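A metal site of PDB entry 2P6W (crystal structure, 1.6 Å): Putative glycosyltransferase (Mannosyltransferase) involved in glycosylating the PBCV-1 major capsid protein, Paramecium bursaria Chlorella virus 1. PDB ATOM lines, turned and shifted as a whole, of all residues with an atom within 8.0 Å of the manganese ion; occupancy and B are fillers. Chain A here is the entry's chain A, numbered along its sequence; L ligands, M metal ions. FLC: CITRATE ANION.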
ATOM      1  N   TYR A  21      -5.171   8.206   2.730  1.00  0.00           N
ATOM      2  CA  TYR A  21      -5.888   9.452   3.035  1.00  0.00           C
ATOM      3  C   TYR A  21      -7.390   9.290   2.904  1.00  0.00           C
ATOM      4  O   TYR A  21      -8.143   9.865   3.687  1.00  0.00           O
ATOM      5  CB  TYR A  21      -5.413  10.628   2.184  1.00  0.00           C
ATOM      6  CG  TYR A  21      -5.932  10.657   0.771  1.00  0.00           C
ATOM      7  CD1 TYR A  21      -7.219  11.164   0.476  1.00  0.00           C
ATOM      8  CD2 TYR A  21      -5.127  10.237  -0.287  1.00  0.00           C
ATOM      9  CE1 TYR A  21      -7.700  11.196  -0.837  1.00  0.00           C
ATOM     10  CE2 TYR A  21      -5.591  10.285  -1.600  1.00  0.00           C
ATOM     11  CZ  TYR A  21      -6.874  10.767  -1.869  1.00  0.00           C
ATOM     12  OH  TYR A  21      -7.306  10.813  -3.185  1.00  0.00           O
ATOM     13  N   HIS A  56     -14.688  11.382 -12.771  1.00  0.00           N
ATOM     14  CA  HIS A  56     -15.256  12.607 -12.195  1.00  0.00           C
ATOM     15  C   HIS A  56     -16.789  12.528 -12.160  1.00  0.00           C
ATOM     16  O   HIS A  56     -17.416  12.922 -11.165  1.00  0.00           O
ATOM     17  CB  HIS A  56     -14.789  13.832 -12.962  1.00  0.00           C
ATOM     18  CG  HIS A  56     -15.124  15.110 -12.276  1.00  0.00           C
ATOM     19  ND1 HIS A  56     -16.362  15.700 -12.369  1.00  0.00           N
ATOM     20  CD2 HIS A  56     -14.397  15.878 -11.433  1.00  0.00           C
ATOM     21  CE1 HIS A  56     -16.369  16.806 -11.649  1.00  0.00           C
ATOM     22  NE2 HIS A  56     -15.188  16.935 -11.060  1.00  0.00           N
ATOM     23  N   ARG A  59     -19.760  10.532  -9.295  1.00  0.00           N
ATOM     24  CA  ARG A  59     -20.587  11.061  -8.198  1.00  0.00           C
ATOM     25  C   ARG A  59     -22.096  11.113  -8.553  1.00  0.00           C
ATOM     26  O   ARG A  59     -22.944  10.919  -7.688  1.00  0.00           O
ATOM     27  CB  ARG A  59     -20.097  12.446  -7.798  1.00  0.00           C
ATOM     28  CG  ARG A  59     -20.240  13.468  -8.881  1.00  0.00           C
ATOM     29  CD  ARG A  59     -19.396  14.711  -8.540  1.00  0.00           C
ATOM     30  NE  ARG A  59     -17.988  14.394  -8.781  1.00  0.00           N
ATOM     31  CZ  ARG A  59     -16.968  15.120  -8.316  1.00  0.00           C
ATOM     32  NH1 ARG A  59     -17.199  16.194  -7.584  1.00  0.00           N
ATOM     33  NH2 ARG A  59     -15.725  14.736  -8.589  1.00  0.00           N
ATOM     34  N   TRP A  78     -22.803  15.394  -1.587  1.00  0.00           N
ATOM     35  CA  TRP A  78     -21.614  14.716  -2.131  1.00  0.00           C
ATOM     36  C   TRP A  78     -20.353  15.378  -1.565  1.00  0.00           C
ATOM     37  O   TRP A  78     -20.241  16.595  -1.627  1.00  0.00           O
ATOM     38  CB  TRP A  78     -21.554  14.850  -3.662  1.00  0.00           C
ATOM     39  CG  TRP A  78     -20.218  14.411  -4.155  1.00  0.00           C
ATOM     40  CD1 TRP A  78     -19.143  15.210  -4.457  1.00  0.00           C
ATOM     41  CD2 TRP A  78     -19.767  13.066  -4.310  1.00  0.00           C
ATOM     42  NE1 TRP A  78     -18.059  14.441  -4.800  1.00  0.00           N
ATOM     43  CE2 TRP A  78     -18.415  13.120  -4.728  1.00  0.00           C
ATOM     44  CE3 TRP A  78     -20.370  11.810  -4.144  1.00  0.00           C
ATOM     45  CZ2 TRP A  78     -17.651  11.958  -4.965  1.00  0.00           C
ATOM     46  CZ3 TRP A  78     -19.615  10.651  -4.404  1.00  0.00           C
ATOM     47  CH2 TRP A  78     -18.268  10.741  -4.798  1.00  0.00           C
ATOM     48  N   LEU A  79     -19.423  14.570  -1.042  1.00  0.00           N
ATOM     49  CA  LEU A  79     -18.077  15.037  -0.685  1.00  0.00           C
ATOM     50  C   LEU A  79     -17.036  14.209  -1.408  1.00  0.00           C
ATOM     51  O   LEU A  79     -17.073  12.961  -1.347  1.00  0.00           O
ATOM     52  CB  LEU A  79     -17.830  14.852   0.824  1.00  0.00           C
ATOM     53  CG  LEU A  79     -18.787  15.554   1.773  1.00  0.00           C
ATOM     54  CD1 LEU A  79     -18.370  15.243   3.214  1.00  0.00           C
ATOM     55  CD2 LEU A  79     -18.916  17.055   1.542  1.00  0.00           C
ATOM     56  N   ASP A  80     -16.092  14.869  -2.096  1.00  0.00           N
ATOM     57  CA  ASP A  80     -14.940  14.160  -2.683  1.00  0.00           C
ATOM     58  C   ASP A  80     -14.243  13.384  -1.582  1.00  0.00           C
ATOM     59  O   ASP A  80     -14.277  13.774  -0.414  1.00  0.00           O
ATOM     60  CB  ASP A  80     -13.910  15.143  -3.243  1.00  0.00           C
ATOM     61  CG  ASP A  80     -14.300  15.741  -4.583  1.00  0.00           C
ATOM     62  OD1 ASP A  80     -15.390  15.409  -5.109  1.00  0.00           O
ATOM     63  OD2 ASP A  80     -13.501  16.543  -5.117  1.00  0.00           O
ATOM     64  N   SER A  81     -13.570  12.294  -1.943  1.00  0.00           N
ATOM     65  CA  SER A  81     -12.797  11.552  -0.935  1.00  0.00           C
ATOM     66  C   SER A  81     -11.577  12.334  -0.440  1.00  0.00           C
ATOM     67  O   SER A  81     -10.919  11.923   0.529  1.00  0.00           O
ATOM     68  CB  SER A  81     -12.357  10.189  -1.482  1.00  0.00           C
ATOM     69  OG  SER A  81     -11.655  10.340  -2.711  1.00  0.00           O
ATOM     70  N   ASP A  82     -11.296  13.483  -1.065  1.00  0.00           N
ATOM     71  CA  ASP A  82     -10.219  14.355  -0.594  1.00  0.00           C
ATOM     72  C   ASP A  82     -10.789  15.534   0.248  1.00  0.00           C
ATOM     73  O   ASP A  82     -10.105  16.528   0.506  1.00  0.00           O
ATOM     74  CB  ASP A  82      -9.387  14.826  -1.768  1.00  0.00           C
ATOM     75  CG  ASP A  82     -10.221  15.202  -2.984  1.00  0.00           C
ATOM     76  OD1 ASP A  82     -10.398  14.340  -3.886  1.00  0.00           O
ATOM     77  OD2 ASP A  82     -10.719  16.333  -3.040  1.00  0.00           O
ATOM     78  N   VAL A  83     -12.029  15.377   0.718  1.00  0.00           N
ATOM     79  CA  VAL A  83     -12.625  16.350   1.630  1.00  0.00           C
ATOM     80  C   VAL A  83     -12.767  15.698   3.017  1.00  0.00           C
ATOM     81  O   VAL A  83     -13.111  14.524   3.107  1.00  0.00           O
ATOM     82  CB  VAL A  83     -14.028  16.816   1.123  1.00  0.00           C
ATOM     83  CG1 VAL A  83     -14.734  17.640   2.183  1.00  0.00           C
ATOM     84  CG2 VAL A  83     -13.899  17.625  -0.169  1.00  0.00           C
ATOM     85  N   ASN A 121     -16.896  24.904  -7.555  1.00  0.00           N
ATOM     86  CA  ASN A 121     -16.127  23.700  -7.287  1.00  0.00           C
ATOM     87  C   ASN A 121     -17.054  22.669  -6.656  1.00  0.00           C
ATOM     88  O   ASN A 121     -17.564  22.888  -5.555  1.00  0.00           O
ATOM     89  CB  ASN A 121     -14.972  24.042  -6.346  1.00  0.00           C
ATOM     90  CG  ASN A 121     -14.130  22.843  -6.012  1.00  0.00           C
ATOM     91  OD1 ASN A 121     -14.607  21.877  -5.405  1.00  0.00           O
ATOM     92  ND2 ASN A 121     -12.833  22.924  -6.333  1.00  0.00           N
ATOM     93  N   THR A 122     -17.281  21.557  -7.370  1.00  0.00           N
ATOM     94  CA  THR A 122     -18.307  20.595  -6.958  1.00  0.00           C
ATOM     95  C   THR A 122     -17.741  19.456  -6.100  1.00  0.00           C
ATOM     96  O   THR A 122     -18.391  18.415  -5.961  1.00  0.00           O
ATOM     97  CB  THR A 122     -19.076  20.017  -8.173  1.00  0.00           C
ATOM     98  OG1 THR A 122     -18.149  19.507  -9.130  1.00  0.00           O
ATOM     99  CG2 THR A 122     -19.983  21.094  -8.810  1.00  0.00           C
ATOM    100  N   GLY A 123     -16.577  19.691  -5.492  1.00  0.00           N
ATOM    101  CA  GLY A 123     -16.005  18.741  -4.520  1.00  0.00           C
ATOM    102  C   GLY A 123     -16.904  18.605  -3.293  1.00  0.00           C
ATOM    103  O   GLY A 123     -16.839  17.617  -2.562  1.00  0.00           O
ATOM    104  N   VAL A 124     -17.744  19.621  -3.078  1.00  0.00           N
ATOM    105  CA  VAL A 124     -18.819  19.629  -2.065  1.00  0.00           C
ATOM    106  C   VAL A 124     -20.059  20.147  -2.787  1.00  0.00           C
ATOM    107  O   VAL A 124     -20.023  21.236  -3.349  1.00  0.00           O
ATOM    108  CB  VAL A 124     -18.507  20.573  -0.891  1.00  0.00           C
ATOM    109  CG1 VAL A 124     -19.639  20.530   0.118  1.00  0.00           C
ATOM    110  CG2 VAL A 124     -17.187  20.147  -0.200  1.00  0.00           C
ATOM    111  N   GLN A 154     -18.522  19.059 -13.163  1.00  0.00           N
ATOM    112  CA  GLN A 154     -18.521  20.413 -12.629  1.00  0.00           C
ATOM    113  C   GLN A 154     -19.009  21.410 -13.694  1.00  0.00           C
ATOM    114  O   GLN A 154     -19.801  22.317 -13.410  1.00  0.00           O
ATOM    115  CB  GLN A 154     -17.113  20.750 -12.174  1.00  0.00           C
ATOM    116  CG  GLN A 154     -16.957  22.109 -11.547  1.00  0.00           C
ATOM    117  CD  GLN A 154     -15.602  22.231 -10.891  1.00  0.00           C
ATOM    118  OE1 GLN A 154     -15.390  21.726  -9.790  1.00  0.00           O
ATOM    119  NE2 GLN A 154     -14.670  22.914 -11.554  1.00  0.00           N
ATOM    120  N   ASN A 178     -16.551  24.441   1.573  1.00  0.00           N
ATOM    121  CA  ASN A 178     -15.680  23.837   0.560  1.00  0.00           C
ATOM    122  C   ASN A 178     -14.349  24.551   0.665  1.00  0.00           C
ATOM    123  O   ASN A 178     -13.907  25.252  -0.255  1.00  0.00           O
ATOM    124  CB  ASN A 178     -16.305  23.955  -0.839  1.00  0.00           C
ATOM    125  CG  ASN A 178     -15.580  23.098  -1.880  1.00  0.00           C
ATOM    126  OD1 ASN A 178     -14.499  22.561  -1.632  1.00  0.00           O
ATOM    127  ND2 ASN A 178     -16.200  22.948  -3.056  1.00  0.00           N
ATOM    128  N   ILE A 180     -10.982  24.953   0.377  1.00  0.00           N
ATOM    129  CA  ILE A 180      -9.796  24.476  -0.316  1.00  0.00           C
ATOM    130  C   ILE A 180      -8.537  24.864   0.462  1.00  0.00           C
ATOM    131  O   ILE A 180      -8.330  26.048   0.777  1.00  0.00           O
ATOM    132  CB  ILE A 180      -9.763  25.005  -1.765  1.00  0.00           C
ATOM    133  CG1 ILE A 180     -10.926  24.412  -2.581  1.00  0.00           C
ATOM    134  CG2 ILE A 180      -8.427  24.706  -2.437  1.00  0.00           C
ATOM    135  CD1 ILE A 180     -11.120  25.042  -3.949  1.00  0.00           C
ATOM    136  N   HIS A 195     -11.074  20.922   2.031  1.00  0.00           N
ATOM    137  CA  HIS A 195     -10.958  20.242   0.743  1.00  0.00           C
ATOM    138  C   HIS A 195      -9.498  20.226   0.255  1.00  0.00           C
ATOM    139  O   HIS A 195      -8.934  21.272  -0.028  1.00  0.00           O
ATOM    140  CB  HIS A 195     -11.903  20.923  -0.258  1.00  0.00           C
ATOM    141  CG  HIS A 195     -11.913  20.303  -1.623  1.00  0.00           C
ATOM    142  ND1 HIS A 195     -12.649  20.824  -2.667  1.00  0.00           N
ATOM    143  CD2 HIS A 195     -11.301  19.197  -2.116  1.00  0.00           C
ATOM    144  CE1 HIS A 195     -12.487  20.068  -3.736  1.00  0.00           C
ATOM    145  NE2 HIS A 195     -11.667  19.080  -3.433  1.00  0.00           N
ATOM    146  N   MET A 196      -8.890  19.049   0.248  1.00  0.00           N
ATOM    147  CA  MET A 196      -7.503  18.921  -0.215  1.00  0.00           C
ATOM    148  C   MET A 196      -7.442  18.862  -1.745  1.00  0.00           C
ATOM    149  O   MET A 196      -6.995  17.876  -2.334  1.00  0.00           O
ATOM    150  CB  MET A 196      -6.852  17.665   0.400  1.00  0.00           C
ATOM    151  CG  MET A 196      -6.836  17.652   1.936  1.00  0.00           C
ATOM    152  SD  MET A 196      -6.127  16.094   2.553  1.00  0.00           S
ATOM    153  CE  MET A 196      -7.351  14.916   1.970  1.00  0.00           C
ATOM    154  N   CYS A 197      -7.854  19.950  -2.376  1.00  0.00           N
ATOM    155  CA  CYS A 197      -8.050  19.984  -3.818  1.00  0.00           C
ATOM    156  C   CYS A 197      -6.736  20.108  -4.577  1.00  0.00           C
ATOM    157  O   CYS A 197      -5.876  20.904  -4.198  1.00  0.00           O
ATOM    158  CB  CYS A 197      -8.960  21.155  -4.140  1.00  0.00           C
ATOM    159  SG  CYS A 197      -9.541  21.239  -5.834  1.00  0.00           S
ATOM    160  N   GLY A 198      -6.568  19.295  -5.625  1.00  0.00           N
ATOM    161  CA  GLY A 198      -5.454  19.464  -6.577  1.00  0.00           C
ATOM    162  C   GLY A 198      -4.125  18.904  -6.150  1.00  0.00           C
ATOM    163  O   GLY A 198      -3.127  19.035  -6.881  1.00  0.00           O
ATOM    164  N   THR A 199      -4.090  18.239  -5.005  1.00  0.00           N
ATOM    165  CA  THR A 199      -2.832  17.716  -4.465  1.00  0.00           C
ATOM    166  C   THR A 199      -2.716  16.212  -4.733  1.00  0.00           C
ATOM    167  O   THR A 199      -3.689  15.556  -5.096  1.00  0.00           O
ATOM    168  CB  THR A 199      -2.730  17.999  -2.962  1.00  0.00           C
ATOM    169  OG1 THR A 199      -3.885  17.481  -2.310  1.00  0.00           O
ATOM    170  CG2 THR A 199      -2.676  19.515  -2.724  1.00  0.00           C
ATOM    171  N   ARG A 204      -1.656  14.282   0.281  1.00  0.00           N
ATOM    172  CA  ARG A 204      -2.871  14.068   1.075  1.00  0.00           C
ATOM    173  C   ARG A 204      -2.690  13.138   2.274  1.00  0.00           C
ATOM    174  O   ARG A 204      -3.262  13.396   3.346  1.00  0.00           O
ATOM    175  CB  ARG A 204      -3.969  13.553   0.145  1.00  0.00           C
ATOM    176  CG  ARG A 204      -4.429  14.621  -0.834  1.00  0.00           C
ATOM    177  CD  ARG A 204      -5.344  14.065  -1.907  1.00  0.00           C
ATOM    178  NE  ARG A 204      -5.934  15.131  -2.726  1.00  0.00           N
ATOM    179  CZ  ARG A 204      -6.590  14.914  -3.866  1.00  0.00           C
ATOM    180  NH1 ARG A 204      -6.772  13.684  -4.323  1.00  0.00           N
ATOM    181  NH2 ARG A 204      -7.105  15.943  -4.529  1.00  0.00           N
HETATM  182  CAC FLC L   1     -11.637  18.462  -7.800  1.00  0.00           C
HETATM  183  CA  FLC L   1     -10.978  17.182  -8.358  1.00  0.00           C
HETATM  184  CB  FLC L   1     -10.267  16.505  -7.219  1.00  0.00           C
HETATM  185  CBC FLC L   1      -9.043  17.154  -6.659  1.00  0.00           C
HETATM  186  CG  FLC L   1      -9.550  15.474  -8.170  1.00  0.00           C
HETATM  187  CGC FLC L   1      -8.782  14.321  -7.497  1.00  0.00           C
HETATM  188  OA1 FLC L   1     -11.903  19.375  -8.589  1.00  0.00           O
HETATM  189  OA2 FLC L   1     -11.852  18.503  -6.557  1.00  0.00           O
HETATM  190  OB1 FLC L   1      -9.211  17.495  -5.479  1.00  0.00           O
HETATM  191  OB2 FLC L   1      -8.030  17.359  -7.368  1.00  0.00           O
HETATM  192  OG1 FLC L   1      -8.573  14.409  -6.280  1.00  0.00           O
HETATM  193  OG2 FLC L   1      -8.405  13.347  -8.217  1.00  0.00           O
HETATM  194  OHB FLC L   1     -11.032  15.521  -6.502  1.00  0.00           O
HETATM  195 MN    MN M   1     -11.480  17.190  -4.768  1.00  0.00          MN
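The manganese ion is bound by OD2 of Asp 82 (2.1 Å), OD2 of Asp 80 (2.2 Å), OA2 of the ligand (2.3 Å), NE2 of His 195 (2.3 Å), OB1 of the ligand (2.4 Å) and OHB of the ligand (2.4 Å). The manganese ion has six donor atoms within binding distance.
The guanidinium group (NH1) of Arg 204 is in salt-bridge range of the side-chain carboxylate (OD1) of Asp 82 (3.7 Å). N of Met 196 lies within hydrogen-bond range of O of Asp 82, 2.8 Å away. The backbone carbonyl oxygen of Gly 123 sits at hydrogen-bond distance from the backbone NH of Asp 80 (2.9 Å). The guanidinium group of Arg 59 is in salt-bridge range of the side-chain carboxylate of Asp 80 (3.2 Å). The indole nitrogen (NE1) of Trp 78 is in hydrogen-bond range of the side-chain carboxylate (OD1) of Asp 80, at 2.9 Å. The side-chain amide oxygen (OD1) of Asn 178 is in hydrogen-bond range of a ring nitrogen (ND1) of His 195 (2.7 Å).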
